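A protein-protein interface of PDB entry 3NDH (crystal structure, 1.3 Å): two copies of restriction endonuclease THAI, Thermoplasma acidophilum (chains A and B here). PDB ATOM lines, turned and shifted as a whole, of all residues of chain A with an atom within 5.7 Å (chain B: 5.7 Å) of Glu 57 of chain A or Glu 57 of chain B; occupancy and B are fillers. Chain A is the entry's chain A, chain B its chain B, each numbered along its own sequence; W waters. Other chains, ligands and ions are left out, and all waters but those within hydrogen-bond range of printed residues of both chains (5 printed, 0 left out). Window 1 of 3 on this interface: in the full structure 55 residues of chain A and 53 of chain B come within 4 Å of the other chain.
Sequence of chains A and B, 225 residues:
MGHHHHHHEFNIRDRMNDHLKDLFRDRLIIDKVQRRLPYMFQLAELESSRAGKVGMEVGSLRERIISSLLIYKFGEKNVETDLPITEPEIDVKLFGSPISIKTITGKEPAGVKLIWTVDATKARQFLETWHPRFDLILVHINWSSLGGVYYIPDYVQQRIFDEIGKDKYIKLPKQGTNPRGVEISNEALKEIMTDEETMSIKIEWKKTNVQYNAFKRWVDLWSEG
The backbone carbonyl oxygen (O) of Ser 48 of chain B sits at hydrogen-bond distance from the backbone NH (N) of Gly 55 of chain B (2.8 Å).
O of Ser 48 of chain A sits at hydrogen-bond distance from N of Gly 55 of chain A.
Among the printed residues, merely in contact across the chains: Glu 57 of chain A with Ile 85 of chain B (3.4 Å), Ile 85 of chain A with Glu 57 of chain B (3.4 Å), Glu 57 of chain A with Glu 57 of chain B (3.6 Å), Glu 57 of chain A with Ser 60 of chain B (3.7 Å), Ser 60 of chain A with Glu 57 of chain B (3.7 Å), Ile 85 of chain A with Gly 55 of chain B (3.8 Å), Gly 55 of chain A with Ile 85 of chain B (3.8 Å), Ser 49 of chain A with Ile 85 of chain B (3.8 Å), Arg 64 of chain A with Ser 48 of chain B (3.9 Å), Ile 85 of chain A with Ser 49 of chain B (3.9 Å), Ser 48 of chain A with Ile 85 of chain B (3.9 Å), Ile 85 of chain A with Ser 48 of chain B (3.9 Å) and Arg 64 of chain A with Ser 49 of chain B (3.98 Å).
Of chain B, only Glu 57 (3.6 Å), Ser 60 (3.7 Å) and Ile 85 (3.4 Å) come within 4 Å of Glu 57 of chain A.
Of chain A, only Glu 57, Ser 60 and Ile 85 come within 4 Å of Glu 57 of chain B.
Printed residues of chain A within 4 Å of Ser 49 of chain B: Arg 64 (3.98 Å) and Ile 85 (3.9 Å).
Of the printed residues of chain B, Ser 60 of chain A touches Glu 57.
Of the printed residues of chain A, Ser 60 of chain B touches Glu 57 (3.7 Å).
Hydrophobic or aromatic side chains of chain A within 4 Å of the printed part of chain B: Ile 85.
Of the 11 printed residues of chain B, 6 touch a printed residue of chain A.
Hydrophobic or aromatic side chains of chain B that line the printed part of chain A: Ile 85.
Ser 48 of chain A touches Ile 85 of chain B, and with the chains exchanged Ile 85 of chain A touches Ser 48 of chain B.
Gly 55 of chain A touches Ile 85 of chain B, and with the chains exchanged Ile 85 of chain A touches Gly 55 of chain B.
Glu 57 of chain A touches Ser 60 of chain B, and with the chains exchanged Ser 60 of chain A touches Glu 57 of chain B.
Glu 57 of chain A touches Ile 85 of chain B, and with the chains exchanged Ile 85 of chain A touches Glu 57 of chain B.
Of the 13 pairs that touch across the chains among the printed residues, 11 have their exchanged pair printed and touching as well.
Water W3 lies within hydrogen-bond range of NH2 of Arg 64 of chain A (2.9 Å), O of Ser 49 of chain B (3.0 Å) and N of Ser 48 of chain B (3.4 Å).
Water W5 bridges the guanidinium group of Arg 64 of chain A (2.9 Å) and the backbone carbonyl oxygen of Ser 49 of chain B (3.0 Å).
Water W4 bridges OG of Ser 60 of chain A (2.9 Å) and OE1 of Glu 57 of chain B (3.1 Å).
Water W2 lies within hydrogen-bond range of the side-chain hydroxyl (OG) of Ser 60 of chain B (2.9 Å) and the side-chain carboxylate (OE1) of Glu 57 of chain A (3.1 Å).
Water W1 bridges NH2 of Arg 64 of chain A (2.9 Å) and O of Ser 49 of chain B (3.0 Å).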
ATOM      1  N   SER A  48      14.416  25.659  34.776  1.00  0.00           N
ATOM      2  CA  SER A  48      14.812  24.344  34.305  1.00  0.00           C
ATOM      3  C   SER A  48      14.089  23.234  35.047  1.00  0.00           C
ATOM      4  O   SER A  48      14.664  22.178  35.271  1.00  0.00           O
ATOM      5  CB  SER A  48      16.301  24.123  34.527  1.00  0.00           C
ATOM      6  OG  SER A  48      17.102  25.160  33.983  1.00  0.00           O
ATOM      7  N   SER A  49      12.846  23.489  35.438  1.00  0.00           N
ATOM      8  CA  SER A  49      12.084  22.543  36.246  1.00  0.00           C
ATOM      9  C   SER A  49      10.715  22.254  35.632  1.00  0.00           C
ATOM     10  O   SER A  49      10.338  22.831  34.607  1.00  0.00           O
ATOM     11  CB  SER A  49      11.898  23.100  37.658  1.00  0.00           C
ATOM     12  OG  SER A  49      13.141  23.208  38.334  1.00  0.00           O
ATOM     13  N   GLY A  55      15.315  19.576  36.239  1.00  0.00           N
ATOM     14  CA  GLY A  55      15.816  18.749  35.151  1.00  0.00           C
ATOM     15  C   GLY A  55      17.346  18.804  35.091  1.00  0.00           C
ATOM     16  O   GLY A  55      18.019  19.731  35.516  1.00  0.00           O
ATOM     17  N   MET A  56      17.903  17.740  34.528  1.00  0.00           N
ATOM     18  CA  MET A  56      19.346  17.637  34.298  1.00  0.00           C
ATOM     19  C   MET A  56      19.873  18.804  33.505  1.00  0.00           C
ATOM     20  O   MET A  56      21.020  19.239  33.725  1.00  0.00           O
ATOM     21  CB  MET A  56      19.670  16.336  33.538  1.00  0.00           C
ATOM     22  CG  MET A  56      19.489  15.111  34.390  1.00  0.00           C
ATOM     23  SD  MET A  56      19.772  13.591  33.505  1.00  0.00           S
ATOM     24  CE  MET A  56      21.521  13.665  33.220  1.00  0.00           C
ATOM     25  N   GLU A  57      19.034  19.361  32.630  1.00  0.00           N
ATOM     26  CA  GLU A  57      19.430  20.461  31.784  1.00  0.00           C
ATOM     27  C   GLU A  57      19.726  21.736  32.571  1.00  0.00           C
ATOM     28  O   GLU A  57      20.292  22.685  32.021  1.00  0.00           O
ATOM     29  CB  GLU A  57      18.402  20.701  30.671  1.00  0.00           C
ATOM     30  CG  GLU A  57      17.087  21.254  31.112  1.00  0.00           C
ATOM     31  CD  GLU A  57      16.045  20.228  31.498  1.00  0.00           C
ATOM     32  OE1 GLU A  57      16.381  19.088  31.854  1.00  0.00           O
ATOM     33  OE2 GLU A  57      14.833  20.592  31.459  1.00  0.00           O
ATOM     34  N   VAL A  58      19.378  21.785  33.849  1.00  0.00           N
ATOM     35  CA  VAL A  58      19.828  22.896  34.701  1.00  0.00           C
ATOM     36  C   VAL A  58      21.324  23.078  34.622  1.00  0.00           C
ATOM     37  O   VAL A  58      21.809  24.196  34.760  1.00  0.00           O
ATOM     38  CB  VAL A  58      19.372  22.705  36.168  1.00  0.00           C
ATOM     39  CG1 VAL A  58      20.178  21.601  36.874  1.00  0.00           C
ATOM     40  CG2 VAL A  58      19.417  24.031  36.935  1.00  0.00           C
ATOM     41  N   GLY A  59      22.069  21.999  34.439  1.00  0.00           N
ATOM     42  CA  GLY A  59      23.517  22.075  34.357  1.00  0.00           C
ATOM     43  C   GLY A  59      23.994  22.954  33.226  1.00  0.00           C
ATOM     44  O   GLY A  59      25.002  23.657  33.342  1.00  0.00           O
ATOM     45  N   SER A  60      23.266  22.940  32.122  1.00  0.00           N
ATOM     46  CA  SER A  60      23.663  23.719  30.965  1.00  0.00           C
ATOM     47  C   SER A  60      23.502  25.211  31.242  1.00  0.00           C
ATOM     48  O   SER A  60      24.316  26.041  30.840  1.00  0.00           O
ATOM     49  CB  SER A  60      22.824  23.256  29.766  1.00  0.00           C
ATOM     50  OG  SER A  60      22.911  21.836  29.560  1.00  0.00           O
ATOM     51  N   LEU A  61      22.460  25.562  31.992  1.00  0.00           N
ATOM     52  CA  LEU A  61      22.249  26.936  32.373  1.00  0.00           C
ATOM     53  C   LEU A  61      23.216  27.408  33.482  1.00  0.00           C
ATOM     54  O   LEU A  61      23.748  28.508  33.440  1.00  0.00           O
ATOM     55  CB  LEU A  61      20.775  27.109  32.760  1.00  0.00           C
ATOM     56  CG  LEU A  61      20.234  28.525  32.925  1.00  0.00           C
ATOM     57  CD1 LEU A  61      20.616  29.450  31.756  1.00  0.00           C
ATOM     58  CD2 LEU A  61      18.715  28.488  33.106  1.00  0.00           C
ATOM     59  N   ARG A  62      23.460  26.561  34.487  1.00  0.00           N
ATOM     60  CA  ARG A  62      24.468  26.871  35.507  1.00  0.00           C
ATOM     61  C   ARG A  62      25.823  27.107  34.859  1.00  0.00           C
ATOM     62  O   ARG A  62      26.566  27.970  35.272  1.00  0.00           O
ATOM     63  CB  ARG A  62      24.585  25.684  36.459  1.00  0.00           C
ATOM     64  CG  ARG A  62      23.398  25.478  37.366  1.00  0.00           C
ATOM     65  CD  ARG A  62      23.603  24.171  38.101  1.00  0.00           C
ATOM     66  NE  ARG A  62      22.490  23.790  38.943  1.00  0.00           N
ATOM     67  CZ  ARG A  62      22.265  22.541  39.348  1.00  0.00           C
ATOM     68  NH1 ARG A  62      23.071  21.574  38.977  1.00  0.00           N
ATOM     69  NH2 ARG A  62      21.220  22.276  40.114  1.00  0.00           N
ATOM     70  N   ARG A  64      26.433  28.387  31.929  1.00  0.00           N
ATOM     71  CA  ARG A  64      26.424  29.755  31.405  1.00  0.00           C
ATOM     72  C   ARG A  64      26.779  30.780  32.471  1.00  0.00           C
ATOM     73  O   ARG A  64      27.498  31.733  32.221  1.00  0.00           O
ATOM     74  CB  ARG A  64      25.061  30.114  30.808  1.00  0.00           C
ATOM     75  CG  ARG A  64      24.772  29.461  29.512  1.00  0.00           C
ATOM     76  CD  ARG A  64      23.679  30.214  28.759  1.00  0.00           C
ATOM     77  NE  ARG A  64      23.095  29.352  27.768  1.00  0.00           N
ATOM     78  CZ  ARG A  64      21.792  29.177  27.601  1.00  0.00           C
ATOM     79  NH1 ARG A  64      20.914  29.863  28.325  1.00  0.00           N
ATOM     80  NH2 ARG A  64      21.377  28.343  26.674  1.00  0.00           N
ATOM     81  N   ILE A  85      27.875  22.687  21.530  1.00  0.00           N
ATOM     82  CA  ILE A  85      27.238  22.267  22.766  1.00  0.00           C
ATOM     83  C   ILE A  85      27.465  20.780  23.069  1.00  0.00           C
ATOM     84  O   ILE A  85      27.417  20.393  24.236  1.00  0.00           O
ATOM     85  CB  ILE A  85      25.724  22.626  22.757  1.00  0.00           C
ATOM     86  CG1 ILE A  85      25.156  22.529  24.152  1.00  0.00           C
ATOM     87  CG2 ILE A  85      24.908  21.716  21.812  1.00  0.00           C
ATOM     88  CD1 ILE A  85      23.863  23.281  24.321  1.00  0.00           C
ATOM     89  N   SER B  48      18.889  27.613  23.772  1.00  0.00           N
ATOM     90  CA  SER B  48      19.259  26.226  24.031  1.00  0.00           C
ATOM     91  C   SER B  48      20.431  25.772  23.188  1.00  0.00           C
ATOM     92  O   SER B  48      20.491  24.613  22.800  1.00  0.00           O
ATOM     93  CB  SER B  48      18.078  25.324  23.741  1.00  0.00           C
ATOM     94  OG  SER B  48      16.926  25.719  24.465  1.00  0.00           O
ATOM     95  N   SER B  49      21.374  26.677  22.930  1.00  0.00           N
ATOM     96  CA  SER B  49      22.478  26.423  22.012  1.00  0.00           C
ATOM     97  C   SER B  49      23.807  26.787  22.629  1.00  0.00           C
ATOM     98  O   SER B  49      23.863  27.407  23.705  1.00  0.00           O
ATOM     99  CB  SER B  49      22.281  27.233  20.731  1.00  0.00           C
ATOM    100  OG  SER B  49      21.201  26.717  19.973  1.00  0.00           O
ATOM    101  N   GLY B  55      21.189  22.181  21.512  1.00  0.00           N
ATOM    102  CA  GLY B  55      21.236  21.079  22.462  1.00  0.00           C
ATOM    103  C   GLY B  55      19.914  20.320  22.484  1.00  0.00           C
ATOM    104  O   GLY B  55      18.846  20.875  22.214  1.00  0.00           O
ATOM    105  N   MET B  56      19.970  19.053  22.897  1.00  0.00           N
ATOM    106  CA  MET B  56      18.773  18.233  23.055  1.00  0.00           C
ATOM    107  C   MET B  56      17.743  18.869  23.998  1.00  0.00           C
ATOM    108  O   MET B  56      16.540  18.694  23.822  1.00  0.00           O
ATOM    109  CB  MET B  56      19.161  16.863  23.612  1.00  0.00           C
ATOM    110  CG  MET B  56      19.900  16.019  22.621  1.00  0.00           C
ATOM    111  SD  MET B  56      20.469  14.455  23.287  1.00  0.00           S
ATOM    112  CE  MET B  56      18.928  13.599  23.464  1.00  0.00           C
ATOM    113  N   GLU B  57      18.235  19.651  24.954  1.00  0.00           N
ATOM    114  CA  GLU B  57      17.352  20.280  25.932  1.00  0.00           C
ATOM    115  C   GLU B  57      16.424  21.293  25.303  1.00  0.00           C
ATOM    116  O   GLU B  57      15.445  21.701  25.940  1.00  0.00           O
ATOM    117  CB  GLU B  57      18.140  20.893  27.101  1.00  0.00           C
ATOM    118  CG  GLU B  57      18.999  22.114  26.766  1.00  0.00           C
ATOM    119  CD  GLU B  57      20.370  21.807  26.271  1.00  0.00           C
ATOM    120  OE1 GLU B  57      20.638  20.683  25.798  1.00  0.00           O
ATOM    121  OE2 GLU B  57      21.212  22.734  26.395  1.00  0.00           O
ATOM    122  N   VAL B  58      16.669  21.690  24.058  1.00  0.00           N
ATOM    123  CA  VAL B  58      15.714  22.543  23.356  1.00  0.00           C
ATOM    124  C   VAL B  58      14.311  21.924  23.392  1.00  0.00           C
ATOM    125  O   VAL B  58      13.307  22.637  23.408  1.00  0.00           O
ATOM    126  CB  VAL B  58      16.157  22.783  21.882  1.00  0.00           C
ATOM    127  CG1 VAL B  58      15.993  21.495  21.053  1.00  0.00           C
ATOM    128  CG2 VAL B  58      15.407  23.943  21.263  1.00  0.00           C
ATOM    129  N   GLY B  59      14.227  20.597  23.415  1.00  0.00           N
ATOM    130  CA  GLY B  59      12.929  19.929  23.438  1.00  0.00           C
ATOM    131  C   GLY B  59      12.125  20.280  24.676  1.00  0.00           C
ATOM    132  O   GLY B  59      10.904  20.390  24.632  1.00  0.00           O
ATOM    133  N   SER B  60      12.792  20.482  25.792  1.00  0.00           N
ATOM    134  CA  SER B  60      12.107  20.787  27.020  1.00  0.00           C
ATOM    135  C   SER B  60      11.497  22.189  26.943  1.00  0.00           C
ATOM    136  O   SER B  60      10.396  22.448  27.440  1.00  0.00           O
ATOM    137  CB  SER B  60      13.120  20.671  28.163  1.00  0.00           C
ATOM    138  OG  SER B  60      13.667  19.347  28.186  1.00  0.00           O
ATOM    139  N   LEU B  61      12.200  23.108  26.294  1.00  0.00           N
ATOM    140  CA  LEU B  61      11.661  24.448  26.117  1.00  0.00           C
ATOM    141  C   LEU B  61      10.546  24.521  25.058  1.00  0.00           C
ATOM    142  O   LEU B  61       9.521  25.178  25.236  1.00  0.00           O
ATOM    143  CB  LEU B  61      12.810  25.417  25.824  1.00  0.00           C
ATOM    144  CG  LEU B  61      12.519  26.905  25.793  1.00  0.00           C
ATOM    145  CD1 LEU B  61      11.637  27.343  26.974  1.00  0.00           C
ATOM    146  CD2 LEU B  61      13.845  27.718  25.752  1.00  0.00           C
ATOM    147  N   ARG B  62      10.709  23.805  23.955  1.00  0.00           N
ATOM    148  CA  ARG B  62       9.640  23.674  22.966  1.00  0.00           C
ATOM    149  C   ARG B  62       8.379  23.118  23.596  1.00  0.00           C
ATOM    150  O   ARG B  62       7.286  23.535  23.281  1.00  0.00           O
ATOM    151  CB  ARG B  62      10.080  22.769  21.830  1.00  0.00           C
ATOM    152  CG  ARG B  62      11.167  23.326  20.935  1.00  0.00           C
ATOM    153  CD  ARG B  62      11.636  22.215  20.037  1.00  0.00           C
ATOM    154  NE  ARG B  62      12.758  22.566  19.185  1.00  0.00           N
ATOM    155  CZ  ARG B  62      13.541  21.659  18.612  1.00  0.00           C
ATOM    156  NH1 ARG B  62      13.363  20.368  18.834  1.00  0.00           N
ATOM    157  NH2 ARG B  62      14.544  22.034  17.833  1.00  0.00           N
ATOM    158  N   ILE B  85       9.291  16.620  36.030  1.00  0.00           N
ATOM    159  CA  ILE B  85      10.021  16.739  34.774  1.00  0.00           C
ATOM    160  C   ILE B  85      10.554  15.389  34.269  1.00  0.00           C
ATOM    161  O   ILE B  85      10.753  15.229  33.056  1.00  0.00           O
ATOM    162  CB  ILE B  85      11.147  17.777  34.901  1.00  0.00           C
ATOM    163  CG1 ILE B  85      11.611  18.214  33.522  1.00  0.00           C
ATOM    164  CG2 ILE B  85      12.307  17.282  35.759  1.00  0.00           C
ATOM    165  CD1 ILE B  85      12.380  19.516  33.542  1.00  0.00           C
HETATM  166  O   HOH W   1      23.460  26.293  26.451  1.00  0.00           O
HETATM  167  O   HOH W   2      16.411  18.565  28.776  1.00  0.00           O
HETATM  168  O   HOH W   3      21.742  29.451  24.070  1.00  0.00           O
HETATM  169  O   HOH W   4      21.008  19.805  28.762  1.00  0.00           O
HETATM  170  O   HOH W   5      25.161  29.055  25.792  1.00  0.00           O
